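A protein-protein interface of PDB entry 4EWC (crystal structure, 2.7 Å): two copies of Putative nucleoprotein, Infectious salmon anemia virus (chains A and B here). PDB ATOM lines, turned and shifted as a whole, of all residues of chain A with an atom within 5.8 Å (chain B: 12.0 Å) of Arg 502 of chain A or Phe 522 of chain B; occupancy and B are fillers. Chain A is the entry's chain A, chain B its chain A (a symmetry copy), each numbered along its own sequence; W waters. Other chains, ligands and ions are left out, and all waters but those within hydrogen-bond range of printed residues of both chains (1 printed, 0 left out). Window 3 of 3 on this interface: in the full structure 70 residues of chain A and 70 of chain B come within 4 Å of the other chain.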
ATOM      1  N   THR A 386     -20.732  16.260  -0.595  1.00  0.00           N
ATOM      2  CA  THR A 386     -21.252  17.420   0.106  1.00  0.00           C
ATOM      3  C   THR A 386     -21.332  18.618  -0.827  1.00  0.00           C
ATOM      4  O   THR A 386     -20.366  18.968  -1.482  1.00  0.00           O
ATOM      5  CB  THR A 386     -20.355  17.798   1.296  1.00  0.00           C
ATOM      6  OG1 THR A 386     -20.135  16.642   2.100  1.00  0.00           O
ATOM      7  CG2 THR A 386     -21.009  18.880   2.139  1.00  0.00           C
ATOM      8  N   THR A 387     -22.489  19.248  -0.869  1.00  0.00           N
ATOM      9  CA  THR A 387     -22.633  20.470  -1.614  1.00  0.00           C
ATOM     10  C   THR A 387     -22.825  21.620  -0.625  1.00  0.00           C
ATOM     11  O   THR A 387     -23.256  21.385   0.492  1.00  0.00           O
ATOM     12  CB  THR A 387     -23.783  20.378  -2.658  1.00  0.00           C
ATOM     13  OG1 THR A 387     -23.942  21.641  -3.301  1.00  0.00           O
ATOM     14  CG2 THR A 387     -25.069  20.044  -2.009  1.00  0.00           C
ATOM     15  N   LYS A 388     -22.474  22.841  -1.040  1.00  0.00           N
ATOM     16  CA  LYS A 388     -22.499  24.048  -0.197  1.00  0.00           C
ATOM     17  C   LYS A 388     -21.972  25.235  -0.993  1.00  0.00           C
ATOM     18  O   LYS A 388     -21.355  25.063  -2.043  1.00  0.00           O
ATOM     19  CB  LYS A 388     -21.602  23.889   1.036  1.00  0.00           C
ATOM     20  CG  LYS A 388     -20.127  23.849   0.673  1.00  0.00           C
ATOM     21  CD  LYS A 388     -19.235  23.919   1.872  1.00  0.00           C
ATOM     22  CE  LYS A 388     -19.239  22.627   2.680  1.00  0.00           C
ATOM     23  NZ  LYS A 388     -18.536  22.785   3.980  1.00  0.00           N
ATOM     24  N   PHE A 390     -19.864  29.265  -0.639  1.00  0.00           N
ATOM     25  CA  PHE A 390     -18.966  30.093   0.145  1.00  0.00           C
ATOM     26  C   PHE A 390     -19.373  31.565   0.021  1.00  0.00           C
ATOM     27  O   PHE A 390     -19.020  32.250  -0.953  1.00  0.00           O
ATOM     28  CB  PHE A 390     -17.522  29.856  -0.288  1.00  0.00           C
ATOM     29  CG  PHE A 390     -17.100  28.425  -0.165  1.00  0.00           C
ATOM     30  CD1 PHE A 390     -16.963  27.831   1.089  1.00  0.00           C
ATOM     31  CD2 PHE A 390     -16.887  27.642  -1.296  1.00  0.00           C
ATOM     32  CE1 PHE A 390     -16.598  26.496   1.210  1.00  0.00           C
ATOM     33  CE2 PHE A 390     -16.522  26.310  -1.176  1.00  0.00           C
ATOM     34  CZ  PHE A 390     -16.378  25.742   0.076  1.00  0.00           C
ATOM     35  N   MET A 413     -19.387  29.074  -5.527  1.00  0.00           N
ATOM     36  CA  MET A 413     -19.344  27.616  -5.495  1.00  0.00           C
ATOM     37  C   MET A 413     -17.919  27.058  -5.520  1.00  0.00           C
ATOM     38  O   MET A 413     -17.600  26.161  -4.747  1.00  0.00           O
ATOM     39  CB  MET A 413     -20.126  27.014  -6.667  1.00  0.00           C
ATOM     40  CG  MET A 413     -21.603  27.376  -6.754  1.00  0.00           C
ATOM     41  SD  MET A 413     -22.758  26.846  -5.261  1.00  0.00           S
ATOM     42  CE  MET A 413     -22.596  24.906  -5.353  1.00  0.00           C
ATOM     43  N   LYS A 414     -17.077  27.584  -6.410  1.00  0.00           N
ATOM     44  CA  LYS A 414     -15.728  27.035  -6.619  1.00  0.00           C
ATOM     45  C   LYS A 414     -14.788  27.190  -5.414  1.00  0.00           C
ATOM     46  O   LYS A 414     -13.985  26.307  -5.142  1.00  0.00           O
ATOM     47  CB  LYS A 414     -15.056  27.624  -7.867  1.00  0.00           C
ATOM     48  CG  LYS A 414     -14.687  29.119  -7.744  1.00  0.00           C
ATOM     49  CD  LYS A 414     -13.804  29.623  -8.895  1.00  0.00           C
ATOM     50  CE  LYS A 414     -13.891  31.147  -9.056  1.00  0.00           C
ATOM     51  NZ  LYS A 414     -13.218  31.940  -7.962  1.00  0.00           N
ATOM     52  N   ASN A 415     -14.883  28.317  -4.720  1.00  0.00           N
ATOM     53  CA  ASN A 415     -14.078  28.585  -3.538  1.00  0.00           C
ATOM     54  C   ASN A 415     -14.557  29.854  -2.832  1.00  0.00           C
ATOM     55  O   ASN A 415     -15.622  30.378  -3.151  1.00  0.00           O
ATOM     56  CB  ASN A 415     -12.583  28.649  -3.864  1.00  0.00           C
ATOM     57  CG  ASN A 415     -12.251  29.678  -4.942  1.00  0.00           C
ATOM     58  OD1 ASN A 415     -12.732  30.819  -4.912  1.00  0.00           O
ATOM     59  ND2 ASN A 415     -11.413  29.280  -5.891  1.00  0.00           N
ATOM     60  N   TYR A 499      -9.271  32.115   2.238  1.00  0.00           N
ATOM     61  CA  TYR A 499     -10.034  30.935   1.813  1.00  0.00           C
ATOM     62  C   TYR A 499      -9.101  29.782   1.459  1.00  0.00           C
ATOM     63  O   TYR A 499      -7.961  29.999   1.066  1.00  0.00           O
ATOM     64  CB  TYR A 499     -10.994  31.277   0.647  1.00  0.00           C
ATOM     65  CG  TYR A 499     -10.311  31.502  -0.680  1.00  0.00           C
ATOM     66  CD1 TYR A 499     -10.078  30.442  -1.534  1.00  0.00           C
ATOM     67  CD2 TYR A 499      -9.893  32.770  -1.074  1.00  0.00           C
ATOM     68  CE1 TYR A 499      -9.448  30.615  -2.728  1.00  0.00           C
ATOM     69  CE2 TYR A 499      -9.256  32.963  -2.284  1.00  0.00           C
ATOM     70  CZ  TYR A 499      -9.037  31.874  -3.111  1.00  0.00           C
ATOM     71  OH  TYR A 499      -8.408  32.016  -4.328  1.00  0.00           O
ATOM     72  N   GLU A 500      -9.580  28.556   1.625  1.00  0.00           N
ATOM     73  CA  GLU A 500      -8.774  27.379   1.295  1.00  0.00           C
ATOM     74  C   GLU A 500      -8.759  27.109  -0.217  1.00  0.00           C
ATOM     75  O   GLU A 500      -9.813  27.067  -0.859  1.00  0.00           O
ATOM     76  CB  GLU A 500      -9.286  26.135   2.041  1.00  0.00           C
ATOM     77  CG  GLU A 500      -8.665  24.818   1.560  1.00  0.00           C
ATOM     78  CD  GLU A 500      -9.079  23.600   2.394  1.00  0.00           C
ATOM     79  OE1 GLU A 500     -10.231  23.522   2.864  1.00  0.00           O
ATOM     80  OE2 GLU A 500      -8.241  22.700   2.587  1.00  0.00           O
ATOM     81  N   ALA A 501      -7.562  26.943  -0.776  1.00  0.00           N
ATOM     82  CA  ALA A 501      -7.439  26.566  -2.173  1.00  0.00           C
ATOM     83  C   ALA A 501      -8.054  25.195  -2.327  1.00  0.00           C
ATOM     84  O   ALA A 501      -7.879  24.341  -1.478  1.00  0.00           O
ATOM     85  CB  ALA A 501      -5.986  26.540  -2.618  1.00  0.00           C
ATOM     86  N   ARG A 502      -8.797  25.003  -3.401  1.00  0.00           N
ATOM     87  CA  ARG A 502      -9.354  23.716  -3.697  1.00  0.00           C
ATOM     88  C   ARG A 502      -8.225  22.850  -4.251  1.00  0.00           C
ATOM     89  O   ARG A 502      -7.550  23.239  -5.191  1.00  0.00           O
ATOM     90  CB  ARG A 502     -10.496  23.878  -4.699  1.00  0.00           C
ATOM     91  CG  ARG A 502     -11.377  22.668  -4.798  1.00  0.00           C
ATOM     92  CD  ARG A 502     -12.412  22.846  -5.873  1.00  0.00           C
ATOM     93  NE  ARG A 502     -13.540  23.667  -5.454  1.00  0.00           N
ATOM     94  CZ  ARG A 502     -14.551  23.234  -4.703  1.00  0.00           C
ATOM     95  NH1 ARG A 502     -14.579  21.983  -4.247  1.00  0.00           N
ATOM     96  NH2 ARG A 502     -15.541  24.057  -4.400  1.00  0.00           N
ATOM     97  N   PRO A 503      -7.998  21.679  -3.646  1.00  0.00           N
ATOM     98  CA  PRO A 503      -6.878  20.824  -4.071  1.00  0.00           C
ATOM     99  C   PRO A 503      -7.151  20.097  -5.397  1.00  0.00           C
ATOM    100  O   PRO A 503      -8.305  19.731  -5.648  1.00  0.00           O
ATOM    101  CB  PRO A 503      -6.760  19.813  -2.934  1.00  0.00           C
ATOM    102  CG  PRO A 503      -8.135  19.750  -2.322  1.00  0.00           C
ATOM    103  CD  PRO A 503      -8.766  21.109  -2.519  1.00  0.00           C
ATOM    104  N   GLU A 504      -6.127  19.901  -6.232  1.00  0.00           N
ATOM    105  CA  GLU A 504      -6.291  19.116  -7.463  1.00  0.00           C
ATOM    106  C   GLU A 504      -5.133  18.147  -7.722  1.00  0.00           C
ATOM    107  O   GLU A 504      -4.836  17.811  -8.877  1.00  0.00           O
ATOM    108  CB  GLU A 504      -6.494  20.026  -8.672  1.00  0.00           C
ATOM    109  N   ASN B 517     -12.822  13.395  14.009  1.00  0.00           N
ATOM    110  CA  ASN B 517     -12.382  13.788  12.673  1.00  0.00           C
ATOM    111  C   ASN B 517     -12.808  15.204  12.311  1.00  0.00           C
ATOM    112  O   ASN B 517     -13.733  15.767  12.895  1.00  0.00           O
ATOM    113  CB  ASN B 517     -12.905  12.824  11.596  1.00  0.00           C
ATOM    114  CG  ASN B 517     -14.361  13.076  11.255  1.00  0.00           C
ATOM    115  OD1 ASN B 517     -15.207  13.199  12.149  1.00  0.00           O
ATOM    116  ND2 ASN B 517     -14.659  13.191   9.971  1.00  0.00           N
ATOM    117  N   VAL B 518     -12.116  15.783  11.344  1.00  0.00           N
ATOM    118  CA  VAL B 518     -12.546  17.056  10.812  1.00  0.00           C
ATOM    119  C   VAL B 518     -12.623  16.927   9.307  1.00  0.00           C
ATOM    120  O   VAL B 518     -12.204  15.922   8.743  1.00  0.00           O
ATOM    121  CB  VAL B 518     -11.619  18.211  11.212  1.00  0.00           C
ATOM    122  CG1 VAL B 518     -11.726  18.433  12.691  1.00  0.00           C
ATOM    123  CG2 VAL B 518     -10.177  17.903  10.835  1.00  0.00           C
ATOM    124  N   THR B 519     -13.206  17.932   8.672  1.00  0.00           N
ATOM    125  CA  THR B 519     -13.223  18.017   7.228  1.00  0.00           C
ATOM    126  C   THR B 519     -12.467  19.259   6.827  1.00  0.00           C
ATOM    127  O   THR B 519     -12.135  20.112   7.671  1.00  0.00           O
ATOM    128  CB  THR B 519     -14.660  18.046   6.644  1.00  0.00           C
ATOM    129  OG1 THR B 519     -15.423  19.138   7.190  1.00  0.00           O
ATOM    130  CG2 THR B 519     -15.360  16.733   6.937  1.00  0.00           C
ATOM    131  N   ASP B 520     -12.164  19.358   5.542  1.00  0.00           N
ATOM    132  CA  ASP B 520     -11.670  20.611   5.037  1.00  0.00           C
ATOM    133  C   ASP B 520     -12.874  21.504   4.740  1.00  0.00           C
ATOM    134  O   ASP B 520     -14.012  21.170   5.094  1.00  0.00           O
ATOM    135  CB  ASP B 520     -10.826  20.379   3.793  1.00  0.00           C
ATOM    136  CG  ASP B 520     -11.620  19.814   2.638  1.00  0.00           C
ATOM    137  OD1 ASP B 520     -12.865  19.701   2.716  1.00  0.00           O
ATOM    138  OD2 ASP B 520     -10.979  19.475   1.617  1.00  0.00           O
ATOM    139  N   SER B 521     -12.627  22.604   4.047  1.00  0.00           N
ATOM    140  CA  SER B 521     -13.678  23.553   3.747  1.00  0.00           C
ATOM    141  C   SER B 521     -14.750  22.992   2.826  1.00  0.00           C
ATOM    142  O   SER B 521     -15.911  23.379   2.891  1.00  0.00           O
ATOM    143  CB  SER B 521     -13.078  24.803   3.123  1.00  0.00           C
ATOM    144  OG  SER B 521     -11.876  25.153   3.781  1.00  0.00           O
ATOM    145  N   PHE B 522     -14.363  22.050   1.980  1.00  0.00           N
ATOM    146  CA  PHE B 522     -15.258  21.548   0.938  1.00  0.00           C
ATOM    147  C   PHE B 522     -16.061  20.354   1.412  1.00  0.00           C
ATOM    148  O   PHE B 522     -17.061  19.966   0.785  1.00  0.00           O
ATOM    149  CB  PHE B 522     -14.419  21.225  -0.300  1.00  0.00           C
ATOM    150  CG  PHE B 522     -13.486  22.338  -0.665  1.00  0.00           C
ATOM    151  CD1 PHE B 522     -13.979  23.494  -1.265  1.00  0.00           C
ATOM    152  CD2 PHE B 522     -12.134  22.280  -0.334  1.00  0.00           C
ATOM    153  CE1 PHE B 522     -13.134  24.544  -1.590  1.00  0.00           C
ATOM    154  CE2 PHE B 522     -11.284  23.354  -0.643  1.00  0.00           C
ATOM    155  CZ  PHE B 522     -11.794  24.481  -1.273  1.00  0.00           C
ATOM    156  N   GLY B 523     -15.640  19.797   2.544  1.00  0.00           N
ATOM    157  CA  GLY B 523     -16.263  18.603   3.077  1.00  0.00           C
ATOM    158  C   GLY B 523     -15.892  17.411   2.216  1.00  0.00           C
ATOM    159  O   GLY B 523     -16.576  16.399   2.218  1.00  0.00           O
ATOM    160  N   GLY B 524     -14.800  17.545   1.473  1.00  0.00           N
ATOM    161  CA  GLY B 524     -14.379  16.523   0.546  1.00  0.00           C
ATOM    162  C   GLY B 524     -13.365  15.581   1.152  1.00  0.00           C
ATOM    163  O   GLY B 524     -13.312  14.402   0.829  1.00  0.00           O
ATOM    164  N   LEU B 525     -12.578  16.115   2.068  1.00  0.00           N
ATOM    165  CA  LEU B 525     -11.440  15.418   2.615  1.00  0.00           C
ATOM    166  C   LEU B 525     -11.563  15.397   4.136  1.00  0.00           C
ATOM    167  O   LEU B 525     -11.969  16.369   4.754  1.00  0.00           O
ATOM    168  CB  LEU B 525     -10.190  16.174   2.191  1.00  0.00           C
ATOM    169  CG  LEU B 525      -8.847  15.638   2.636  1.00  0.00           C
ATOM    170  CD1 LEU B 525      -8.456  14.484   1.750  1.00  0.00           C
ATOM    171  CD2 LEU B 525      -7.827  16.741   2.558  1.00  0.00           C
ATOM    172  N   ALA B 526     -11.226  14.287   4.756  1.00  0.00           N
ATOM    173  CA  ALA B 526     -11.278  14.256   6.204  1.00  0.00           C
ATOM    174  C   ALA B 526      -9.929  13.934   6.827  1.00  0.00           C
ATOM    175  O   ALA B 526      -9.162  13.144   6.285  1.00  0.00           O
ATOM    176  CB  ALA B 526     -12.339  13.294   6.684  1.00  0.00           C
ATOM    177  N   VAL B 527      -9.624  14.589   7.945  1.00  0.00           N
ATOM    178  CA  VAL B 527      -8.490  14.187   8.759  1.00  0.00           C
ATOM    179  C   VAL B 527      -9.072  13.607  10.026  1.00  0.00           C
ATOM    180  O   VAL B 527     -10.044  14.123  10.572  1.00  0.00           O
ATOM    181  CB  VAL B 527      -7.507  15.349   9.059  1.00  0.00           C
ATOM    182  CG1 VAL B 527      -6.436  14.918  10.070  1.00  0.00           C
ATOM    183  CG2 VAL B 527      -6.849  15.798   7.796  1.00  0.00           C
HETATM  184  O   HOH W   1      -8.299  20.521   1.505  1.00  0.00           O
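CB of Thr 386 of chain A touches O of Phe 522 of chain B (3.98 Å). Gly 523 of chain B touches Thr 386 of chain A (O to OG1, 3.6 Å). Phe 522 of chain B touches Lys 388 of chain A (O to CE, 3.9 Å). O of Ser 521 of chain B touches CE1 of Phe 390 of chain A (3.6 Å). Phe 522 of chain B touches Phe 390 of chain A (CD1 to CZ, 3.6 Å). Glu 500 of chain A touches Asp 520 of chain B (OE1 to CB, 3.3 Å). Glu 500 of chain A touches Phe 522 of chain B. Ala 501 of chain A touches Phe 522 of chain B. Arg 502 of chain A touches Phe 522 of chain B (NH1 to CD1, 3.4 Å). Phe 522 of chain B touches Pro 503 of chain A (CE2 to CD, 3.9 Å).
Of chain B, only Phe 522 (3.98 Å) and Gly 523 (3.6 Å) come within 4 Å of Thr 386 of chain A. Lys 388 of chain A touches just these residues of chain B: Ser 521 and Phe 522. Printed residues of chain B within 4 Å of Phe 390 of chain A: Ser 521 and Phe 522. No residue of chain B comes within 4 Å of Met 413 of chain A. Glu 500 of chain A touches just these residues of chain B: Asp 520, Ser 521 and Phe 522. Ala 501 of chain A touches just one residue of chain B: Phe 522. Arg 502 of chain A touches one residue of chain B. Of chain B, only Phe 522 comes within 4 Å of Pro 503 of chain A. Of the printed residues of chain A, Asp 520 of chain B touches Glu 500 (3.3 Å). Of the printed residues of chain A, Ser 521 of chain B touches Lys 388 (2.9 Å), Phe 390 (3.6 Å) and Glu 500 (2.5 Å). Of chain A, only Thr 386 (3.98 Å), Lys 388 (3.9 Å), Phe 390 (3.6 Å), Glu 500 (3.3 Å), Ala 501 (3.6 Å), Arg 502 (3.4 Å) and Pro 503 (3.9 Å) come within 4 Å of Phe 522 of chain B. Of the printed residues of chain A, Gly 523 of chain B touches Thr 386. The nearest residue of chain A that does not touch Phe 522 of chain B is Lys 414 of chain A (4.1 Å). The nearest printed residue of chain B that does not touch Phe 390 of chain A is Gly 523 of chain B (6.5 Å).
Water W1 bridges OE2 of Glu 500 of chain A (2.4 Å) and OD2 of Asp 520 of chain B (2.9 Å).
The backbone carbonyl oxygen of Ser 521 of chain B sits at hydrogen-bond distance from the side-chain amino group of Lys 388 of chain A, 2.9 Å away. OG of Ser 521 of chain B is in hydrogen-bond range of OE1 of Glu 500 of chain A, at 2.5 Å.
Hydrophobic or aromatic side chains of chain B within 4 Å of the printed part of chain A: Phe 522. Printed residues of chain A that touch a printed residue of chain B: Thr 386, Lys 388, Phe 390, Glu 500, Ala 501, Arg 502 and Pro 503. Hydrophobic or aromatic side chains of chain A within 4 Å of the printed part of chain B: Phe 390 and Pro 503. Among the printed residues, no Asp or Glu carboxylate lies within 4 Å of a Lys or Arg side-chain nitrogen of the other chain.
No position is printed for both chains.
The backbone carbonyl oxygen (O) of Met 413 of chain A sits at hydrogen-bond distance from the guanidinium group (NH2) of Arg 502 of chain A (3.0 Å). The backbone carbonyl oxygen of Lys 414 of chain A lies within hydrogen-bond range of the guanidinium group of Arg 502 of chain A, at 2.7 Å. The backbone NH (N) of Phe 522 of chain B is in hydrogen-bond range of the side-chain carboxylate (OD1) of Asp 520 of chain B (2.9 Å). The backbone NH (N) of Gly 523 of chain B lies within hydrogen-bond range of the side-chain carboxylate (OD1) of Asp 520 of chain B (2.8 Å). The side-chain carboxylate (OD1) of Asp 520 of chain B is in hydrogen-bond range of the backbone NH (N) of Gly 524 of chain B. The backbone carbonyl oxygen (O) of Leu 525 of chain B sits at hydrogen-bond distance from the backbone NH (N) of Asp 520 of chain B (3.1 Å).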
